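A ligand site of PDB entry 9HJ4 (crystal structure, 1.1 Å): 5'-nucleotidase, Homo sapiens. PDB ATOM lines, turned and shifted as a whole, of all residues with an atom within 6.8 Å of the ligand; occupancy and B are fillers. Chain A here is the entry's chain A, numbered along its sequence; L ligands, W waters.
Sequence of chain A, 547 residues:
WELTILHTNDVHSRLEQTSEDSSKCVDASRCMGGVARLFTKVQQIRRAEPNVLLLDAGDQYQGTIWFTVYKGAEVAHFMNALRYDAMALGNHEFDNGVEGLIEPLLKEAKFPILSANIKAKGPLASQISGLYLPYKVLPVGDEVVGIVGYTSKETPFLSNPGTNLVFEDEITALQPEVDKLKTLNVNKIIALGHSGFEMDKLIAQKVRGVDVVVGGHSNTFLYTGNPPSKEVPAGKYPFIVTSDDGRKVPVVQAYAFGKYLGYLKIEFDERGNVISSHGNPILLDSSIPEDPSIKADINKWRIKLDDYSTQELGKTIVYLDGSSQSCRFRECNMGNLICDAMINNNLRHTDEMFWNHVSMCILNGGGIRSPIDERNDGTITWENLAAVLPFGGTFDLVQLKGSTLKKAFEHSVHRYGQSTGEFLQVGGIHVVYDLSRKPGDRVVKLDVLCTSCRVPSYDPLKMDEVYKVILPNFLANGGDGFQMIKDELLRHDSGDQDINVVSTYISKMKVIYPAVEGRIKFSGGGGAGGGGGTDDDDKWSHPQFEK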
ATOM      1  N   ASP A  21      15.399  20.307   3.661  1.00  0.00           N
ATOM      2  CA  ASP A  21      16.565  20.972   4.221  1.00  0.00           C
ATOM      3  C   ASP A  21      17.802  20.087   4.196  1.00  0.00           C
ATOM      4  O   ASP A  21      18.806  20.416   4.854  1.00  0.00           O
ATOM      5  CB  ASP A  21      16.279  21.481   5.637  1.00  0.00           C
ATOM      6  CG  ASP A  21      16.171  20.387   6.667  1.00  0.00           C
ATOM      7  OD1 ASP A  21      16.272  19.189   6.312  1.00  0.00           O
ATOM      8  OD2 ASP A  21      15.992  20.727   7.847  1.00  0.00           O
ATOM      9  N   SER A 324      18.381  17.902  28.311  1.00  0.00           N
ATOM     10  CA  SER A 324      18.191  19.347  28.198  1.00  0.00           C
ATOM     11  C   SER A 324      18.339  20.041  29.536  1.00  0.00           C
ATOM     12  O   SER A 324      18.847  21.171  29.606  1.00  0.00           O
ATOM     13  CB  SER A 324      16.841  19.662  27.569  1.00  0.00           C
ATOM     14  OG  SER A 324      15.769  19.215  28.390  1.00  0.00           O
ATOM     15  N   ARG A 328      21.205  22.695  28.548  1.00  0.00           N
ATOM     16  CA  ARG A 328      20.691  24.034  28.321  1.00  0.00           C
ATOM     17  C   ARG A 328      20.863  24.940  29.537  1.00  0.00           C
ATOM     18  O   ARG A 328      20.432  26.089  29.497  1.00  0.00           O
ATOM     19  CB  ARG A 328      19.229  24.008  27.878  1.00  0.00           C
ATOM     20  CG  ARG A 328      19.030  23.198  26.611  1.00  0.00           C
ATOM     21  CD  ARG A 328      17.612  23.318  26.121  1.00  0.00           C
ATOM     22  NE  ARG A 328      17.352  22.381  25.041  1.00  0.00           N
ATOM     23  CZ  ARG A 328      16.315  22.457  24.224  1.00  0.00           C
ATOM     24  NH1 ARG A 328      15.480  23.478  24.263  1.00  0.00           N
ATOM     25  NH2 ARG A 328      16.136  21.503  23.322  1.00  0.00           N
ATOM     26  N   LEU A 363      28.955  24.922  20.748  1.00  0.00           N
ATOM     27  CA  LEU A 363      27.911  23.968  20.384  1.00  0.00           C
ATOM     28  C   LEU A 363      26.652  24.362  21.135  1.00  0.00           C
ATOM     29  O   LEU A 363      26.645  24.379  22.369  1.00  0.00           O
ATOM     30  CB  LEU A 363      28.365  22.552  20.799  1.00  0.00           C
ATOM     31  CG  LEU A 363      27.361  21.419  20.649  1.00  0.00           C
ATOM     32  CD1 LEU A 363      26.942  21.192  19.225  1.00  0.00           C
ATOM     33  CD2 LEU A 363      27.991  20.177  21.283  1.00  0.00           C
ATOM     34  N   ASN A 364      25.579  24.673  20.420  1.00  0.00           N
ATOM     35  CA  ASN A 364      24.330  25.014  21.093  1.00  0.00           C
ATOM     36  C   ASN A 364      23.774  23.791  21.820  1.00  0.00           C
ATOM     37  O   ASN A 364      23.665  22.703  21.247  1.00  0.00           O
ATOM     38  CB  ASN A 364      23.300  25.559  20.096  1.00  0.00           C
ATOM     39  CG  ASN A 364      23.075  24.664  18.869  1.00  0.00           C
ATOM     40  OD1 ASN A 364      24.007  24.332  18.165  1.00  0.00           O
ATOM     41  ND2 ASN A 364      21.829  24.281  18.637  1.00  0.00           N
ATOM     42  N   GLY A 365      23.401  23.969  23.079  1.00  0.00           N
ATOM     43  CA  GLY A 365      22.881  22.869  23.854  1.00  0.00           C
ATOM     44  C   GLY A 365      21.598  22.283  23.292  1.00  0.00           C
ATOM     45  O   GLY A 365      21.329  21.104  23.468  1.00  0.00           O
ATOM     46  N   GLY A 366      20.792  23.115  22.615  1.00  0.00           N
ATOM     47  CA  GLY A 366      19.617  22.618  21.930  1.00  0.00           C
ATOM     48  C   GLY A 366      19.918  21.680  20.783  1.00  0.00           C
ATOM     49  O   GLY A 366      18.980  21.039  20.287  1.00  0.00           O
ATOM     50  N   GLY A 367      21.172  21.608  20.344  1.00  0.00           N
ATOM     51  CA  GLY A 367      21.575  20.658  19.324  1.00  0.00           C
ATOM     52  C   GLY A 367      21.889  19.268  19.850  1.00  0.00           C
ATOM     53  O   GLY A 367      22.127  18.359  19.068  1.00  0.00           O
ATOM     54  N   ILE A 368      21.884  19.109  21.167  1.00  0.00           N
ATOM     55  CA  ILE A 368      22.173  17.838  21.832  1.00  0.00           C
ATOM     56  C   ILE A 368      20.829  17.256  22.239  1.00  0.00           C
ATOM     57  O   ILE A 368      20.132  17.841  23.074  1.00  0.00           O
ATOM     58  CB  ILE A 368      23.076  18.051  23.052  1.00  0.00           C
ATOM     59  CG1 ILE A 368      24.394  18.714  22.633  1.00  0.00           C
ATOM     60  CG2 ILE A 368      23.319  16.743  23.770  1.00  0.00           C
ATOM     61  CD1 ILE A 368      25.253  19.165  23.795  1.00  0.00           C
ATOM     62  N   ARG A 369      20.432  16.134  21.650  1.00  0.00           N
ATOM     63  CA  ARG A 369      19.032  15.726  21.693  1.00  0.00           C
ATOM     64  C   ARG A 369      18.763  14.483  22.508  1.00  0.00           C
ATOM     65  O   ARG A 369      17.596  14.077  22.612  1.00  0.00           O
ATOM     66  CB  ARG A 369      18.504  15.544  20.265  1.00  0.00           C
ATOM     67  CG  ARG A 369      18.612  16.786  19.393  1.00  0.00           C
ATOM     68  CD  ARG A 369      18.025  18.051  19.980  1.00  0.00           C
ATOM     69  NE  ARG A 369      16.588  17.929  20.225  1.00  0.00           N
ATOM     70  CZ  ARG A 369      15.778  18.966  20.383  1.00  0.00           C
ATOM     71  NH1 ARG A 369      16.229  20.195  20.309  1.00  0.00           N
ATOM     72  NH2 ARG A 369      14.482  18.742  20.598  1.00  0.00           N
ATOM     73  N   PHE A 391      20.075  16.024  13.292  1.00  0.00           N
ATOM     74  CA  PHE A 391      19.720  17.080  12.339  1.00  0.00           C
ATOM     75  C   PHE A 391      20.448  16.977  10.993  1.00  0.00           C
ATOM     76  O   PHE A 391      20.109  17.729  10.078  1.00  0.00           O
ATOM     77  CB  PHE A 391      19.954  18.473  12.946  1.00  0.00           C
ATOM     78  CG  PHE A 391      19.090  18.774  14.129  1.00  0.00           C
ATOM     79  CD1 PHE A 391      17.725  18.956  13.990  1.00  0.00           C
ATOM     80  CD2 PHE A 391      19.643  18.899  15.388  1.00  0.00           C
ATOM     81  CE1 PHE A 391      16.945  19.258  15.077  1.00  0.00           C
ATOM     82  CE2 PHE A 391      18.854  19.192  16.483  1.00  0.00           C
ATOM     83  CZ  PHE A 391      17.502  19.355  16.340  1.00  0.00           C
ATOM     84  N   GLY A 392      21.414  16.080  10.843  1.00  0.00           N
ATOM     85  CA  GLY A 392      22.120  15.921   9.583  1.00  0.00           C
ATOM     86  C   GLY A 392      23.089  17.020   9.265  1.00  0.00           C
ATOM     87  O   GLY A 392      23.419  17.226   8.093  1.00  0.00           O
ATOM     88  N   GLY A 393      23.579  17.717  10.290  1.00  0.00           N
ATOM     89  CA  GLY A 393      24.434  18.865  10.095  1.00  0.00           C
ATOM     90  C   GLY A 393      25.906  18.516  10.012  1.00  0.00           C
ATOM     91  O   GLY A 393      26.309  17.360  10.001  1.00  0.00           O
ATOM     92  N   ARG A 415      18.551  35.202  28.119  1.00  0.00           N
ATOM     93  CA  ARG A 415      17.268  34.873  28.728  1.00  0.00           C
ATOM     94  C   ARG A 415      17.378  33.564  29.512  1.00  0.00           C
ATOM     95  O   ARG A 415      16.465  32.742  29.529  1.00  0.00           O
ATOM     96  CB  ARG A 415      16.148  34.820  27.690  1.00  0.00           C
ATOM     97  CG  ARG A 415      16.403  33.852  26.588  1.00  0.00           C
ATOM     98  CD  ARG A 415      15.242  33.737  25.621  1.00  0.00           C
ATOM     99  NE  ARG A 415      15.651  32.877  24.518  1.00  0.00           N
ATOM    100  CZ  ARG A 415      14.839  32.417  23.581  1.00  0.00           C
ATOM    101  NH1 ARG A 415      13.557  32.743  23.561  1.00  0.00           N
ATOM    102  NH2 ARG A 415      15.335  31.619  22.637  1.00  0.00           N
ATOM    103  N   SER A 419      15.240  27.116  29.512  1.00  0.00           N
ATOM    104  CA  SER A 419      15.518  25.885  28.763  1.00  0.00           C
ATOM    105  C   SER A 419      15.500  26.134  27.254  1.00  0.00           C
ATOM    106  O   SER A 419      14.973  25.339  26.485  1.00  0.00           O
ATOM    107  CB  SER A 419      14.575  24.750  29.152  1.00  0.00           C
ATOM    108  OG  SER A 419      15.113  23.508  28.738  1.00  0.00           O
ATOM    109  N   THR A 420      16.114  27.232  26.827  1.00  0.00           N
ATOM    110  CA  THR A 420      16.226  27.541  25.408  1.00  0.00           C
ATOM    111  C   THR A 420      17.533  26.982  24.854  1.00  0.00           C
ATOM    112  O   THR A 420      18.513  26.733  25.564  1.00  0.00           O
ATOM    113  CB  THR A 420      16.126  29.056  25.210  1.00  0.00           C
ATOM    114  OG1 THR A 420      17.143  29.678  26.006  1.00  0.00           O
ATOM    115  CG2 THR A 420      14.746  29.585  25.601  1.00  0.00           C
ATOM    116  N   GLY A 421      17.528  26.768  23.540  1.00  0.00           N
ATOM    117  CA  GLY A 421      18.601  26.001  22.912  1.00  0.00           C
ATOM    118  C   GLY A 421      19.914  26.725  22.713  1.00  0.00           C
ATOM    119  O   GLY A 421      20.912  26.051  22.411  1.00  0.00           O
ATOM    120  N   GLU A 422      19.954  28.053  22.884  1.00  0.00           N
ATOM    121  CA  GLU A 422      21.137  28.830  22.528  1.00  0.00           C
ATOM    122  C   GLU A 422      22.257  28.727  23.552  1.00  0.00           C
ATOM    123  O   GLU A 422      23.346  29.240  23.287  1.00  0.00           O
ATOM    124  CB  GLU A 422      20.803  30.297  22.298  1.00  0.00           C
ATOM    125  CG  GLU A 422      20.297  31.070  23.523  1.00  0.00           C
ATOM    126  CD  GLU A 422      18.784  31.029  23.724  1.00  0.00           C
ATOM    127  OE1 GLU A 422      18.084  30.286  22.989  1.00  0.00           O
ATOM    128  OE2 GLU A 422      18.284  31.753  24.613  1.00  0.00           O
ATOM    129  N   PRO A 472      28.494  24.144  14.838  1.00  0.00           N
ATOM    130  CA  PRO A 472      27.536  23.547  13.892  1.00  0.00           C
ATOM    131  C   PRO A 472      27.235  24.498  12.757  1.00  0.00           C
ATOM    132  O   PRO A 472      27.135  25.708  12.945  1.00  0.00           O
ATOM    133  CB  PRO A 472      26.276  23.340  14.750  1.00  0.00           C
ATOM    134  CG  PRO A 472      26.764  23.309  16.164  1.00  0.00           C
ATOM    135  CD  PRO A 472      27.932  24.230  16.202  1.00  0.00           C
ATOM    136  N   ASN A 473      26.980  23.923  11.568  1.00  0.00           N
ATOM    137  CA  ASN A 473      26.530  24.749  10.458  1.00  0.00           C
ATOM    138  C   ASN A 473      25.283  25.546  10.831  1.00  0.00           C
ATOM    139  O   ASN A 473      25.097  26.680  10.376  1.00  0.00           O
ATOM    140  CB  ASN A 473      26.305  23.918   9.179  1.00  0.00           C
ATOM    141  CG  ASN A 473      25.162  22.898   9.278  1.00  0.00           C
ATOM    142  OD1 ASN A 473      25.124  22.043  10.162  1.00  0.00           O
ATOM    143  ND2 ASN A 473      24.276  22.950   8.300  1.00  0.00           N
ATOM    144  N   PHE A 474      24.418  24.974  11.673  1.00  0.00           N
ATOM    145  CA  PHE A 474      23.227  25.679  12.133  1.00  0.00           C
ATOM    146  C   PHE A 474      23.563  27.014  12.760  1.00  0.00           C
ATOM    147  O   PHE A 474      22.842  27.996  12.545  1.00  0.00           O
ATOM    148  CB  PHE A 474      22.505  24.770  13.122  1.00  0.00           C
ATOM    149  CG  PHE A 474      21.326  25.389  13.817  1.00  0.00           C
ATOM    150  CD1 PHE A 474      20.120  25.589  13.161  1.00  0.00           C
ATOM    151  CD2 PHE A 474      21.411  25.715  15.154  1.00  0.00           C
ATOM    152  CE1 PHE A 474      19.037  26.134  13.827  1.00  0.00           C
ATOM    153  CE2 PHE A 474      20.327  26.262  15.834  1.00  0.00           C
ATOM    154  CZ  PHE A 474      19.153  26.460  15.173  1.00  0.00           C
ATOM    155  N   LEU A 475      24.633  27.086  13.557  1.00  0.00           N
ATOM    156  CA  LEU A 475      25.035  28.343  14.169  1.00  0.00           C
ATOM    157  C   LEU A 475      25.779  29.245  13.197  1.00  0.00           C
ATOM    158  O   LEU A 475      25.616  30.480  13.250  1.00  0.00           O
ATOM    159  CB  LEU A 475      25.912  28.102  15.395  1.00  0.00           C
ATOM    160  CG  LEU A 475      25.247  27.406  16.571  1.00  0.00           C
ATOM    161  CD1 LEU A 475      26.195  27.496  17.782  1.00  0.00           C
ATOM    162  CD2 LEU A 475      23.882  27.976  16.878  1.00  0.00           C
ATOM    163  N   GLY A 479      21.485  30.425  13.167  1.00  0.00           N
ATOM    164  CA  GLY A 479      20.422  29.778  13.903  1.00  0.00           C
ATOM    165  C   GLY A 479      20.447  30.142  15.376  1.00  0.00           C
ATOM    166  O   GLY A 479      21.435  30.619  15.918  1.00  0.00           O
ATOM    167  N   ASP A 480      19.318  29.907  16.036  1.00  0.00           N
ATOM    168  CA  ASP A 480      19.196  30.138  17.478  1.00  0.00           C
ATOM    169  C   ASP A 480      19.430  31.608  17.830  1.00  0.00           C
ATOM    170  O   ASP A 480      19.818  31.915  18.956  1.00  0.00           O
ATOM    171  CB  ASP A 480      20.115  29.233  18.299  1.00  0.00           C
ATOM    172  CG  ASP A 480      19.390  28.052  18.890  1.00  0.00           C
ATOM    173  OD1 ASP A 480      18.139  28.046  18.898  1.00  0.00           O
ATOM    174  OD2 ASP A 480      20.065  27.130  19.367  1.00  0.00           O
ATOM    175  N   ASP A 498      28.248  15.730  11.452  1.00  0.00           N
ATOM    176  CA  ASP A 498      28.255  15.762  12.920  1.00  0.00           C
ATOM    177  C   ASP A 498      28.396  14.361  13.533  1.00  0.00           C
ATOM    178  O   ASP A 498      29.287  14.137  14.370  1.00  0.00           O
ATOM    179  CB  ASP A 498      27.047  16.548  13.453  1.00  0.00           C
ATOM    180  CG  ASP A 498      25.676  16.164  12.837  1.00  0.00           C
ATOM    181  OD1 ASP A 498      25.467  15.063  12.304  1.00  0.00           O
ATOM    182  OD2 ASP A 498      24.750  17.013  12.960  1.00  0.00           O
HETATM  183  N1  LIG L   1      20.437  22.434  16.589  1.00  0.00           N
HETATM  184  N2  LIG L   1      19.824  22.059  12.489  1.00  0.00           N
HETATM  185  C1  LIG L   1      19.241  22.622  16.036  1.00  0.00           C
HETATM  186  C2  LIG L   1      21.353  22.096  15.672  1.00  0.00           C
HETATM  187  C3  LIG L   1      19.964  22.147  13.820  1.00  0.00           C
HETATM  188  C4  LIG L   1      18.923  22.506  14.693  1.00  0.00           C
HETATM  189  C5  LIG L   1      17.129  23.065  15.654  1.00  0.00           C
HETATM  190  C6  LIG L   1      15.044  25.080  13.742  1.00  0.00           C
HETATM  191  C7  LIG L   1      18.115  24.721  18.481  1.00  0.00           C
HETATM  192  N3  LIG L   1      18.063  22.976  16.660  1.00  0.00           N
HETATM  193  C8  LIG L   1      16.701  25.099  18.927  1.00  0.00           C
HETATM  194  O1  LIG L   1      16.739  26.088  19.947  1.00  0.00           O
HETATM  195  C9  LIG L   1      16.183  23.799  19.481  1.00  0.00           C
HETATM  196  C10 LIG L   1      14.668  25.174  12.274  1.00  0.00           C
HETATM  197  C11 LIG L   1      13.818  26.363  11.952  1.00  0.00           C
HETATM  198  C12 LIG L   1      14.682  23.705  19.604  1.00  0.00           C
HETATM  199  C13 LIG L   1      17.944  23.242  18.090  1.00  0.00           C
HETATM  200  C14 LIG L   1      14.851  23.678  14.282  1.00  0.00           C
HETATM  201  N4  LIG L   1      21.184  21.939  14.356  1.00  0.00           N
HETATM  202  N5  LIG L   1      17.599  22.800  14.469  1.00  0.00           N
HETATM  203  O2  LIG L   1      14.367  22.454  20.231  1.00  0.00           O
HETATM  204  O3  LIG L   1      11.871  22.590  20.605  1.00  0.00           O
HETATM  205  O4  LIG L   1      13.398  23.486  22.350  1.00  0.00           O
HETATM  206  O5  LIG L   1      13.376  21.010  21.920  1.00  0.00           O
HETATM  207  O6  LIG L   1      16.682  22.816  18.564  1.00  0.00           O
HETATM  208  O7  LIG L   1      19.038  24.787  19.566  1.00  0.00           O
HETATM  209  P1  LIG L   1      13.176  22.397  21.328  1.00  0.00           P
HETATM  210  S1  LIG L   1      15.478  23.475  15.977  1.00  0.00           S
HETATM  211  O   HOH W   1      21.902  21.435  10.600  1.00  0.00           O
HETATM  212  O   HOH W   2      15.167  27.146  21.919  1.00  0.00           O
HETATM  213  O   HOH W   3      12.829  25.973  22.185  1.00  0.00           O
HETATM  214  O   HOH W   4      23.743  21.813  12.762  1.00  0.00           O
HETATM  215  O   HOH W   5      17.002  22.352  11.795  1.00  0.00           O
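The side-chain carboxylate (OD2) of Asp 480 is in hydrogen-bond range of an oxygen (O7) of the ligand, at 2.6 Å. O4 of the ligand is in salt-bridge range of NH1 of Arg 328, 2.8 Å away. NH2 of Arg 369 is in salt-bridge range of O5 of the ligand (2.8 Å). The side-chain amide nitrogen (ND2) of Asn 364 is in hydrogen-bond range of an oxygen (O7) of the ligand (3.0 Å).
The side-chain carboxylate (OD2) of Asp 480 lies within hydrogen-bond range of the side-chain amide nitrogen (ND2) of Asn 364, at 3.4 Å. NH1 of Arg 328 is in hydrogen-bond range of O of Ser 419. The backbone carbonyl oxygen of Gly 366 lies within hydrogen-bond range of the guanidinium group of Arg 369 (2.9 Å). N of Gly 367 sits close to ND2 of Asn 364. N of Gly 366 lies within hydrogen-bond range of O of Gly 421. The backbone carbonyl oxygen (O) of Phe 474 lies within hydrogen-bond range of the backbone NH (N) of Gly 479 (2.9 Å). O of Gly 421 sits at hydrogen-bond distance from N of Gly 365.
The backbone carbonyl oxygen (O) of Gly 366 sits close to an oxygen (O6) of the ligand (3.4 Å). Residues that only touch the ligand: Gly 367 (3.5 Å), Phe 391 (3.5 Å), Gly 421 (3.5 Å) and Phe 474 (3.4 Å). Hydrophobic or aromatic side chains that line the ligand: Phe 391 and Phe 474.
Water W2 bridges an oxygen (O1) of the ligand (2.7 Å) and the backbone NH (N) of Gly 421 (2.9 Å). Water W1 bridges a nitrogen (N2) of the ligand and the side-chain amide oxygen (OD1) of Asn 473. Water W4 lies within hydrogen-bond range of the side-chain amide oxygen (OD1) of Asn 473 (3.0 Å), a nitrogen (N4) of the ligand (3.0 Å) and the backbone NH (N) of Phe 474 (3.4 Å).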
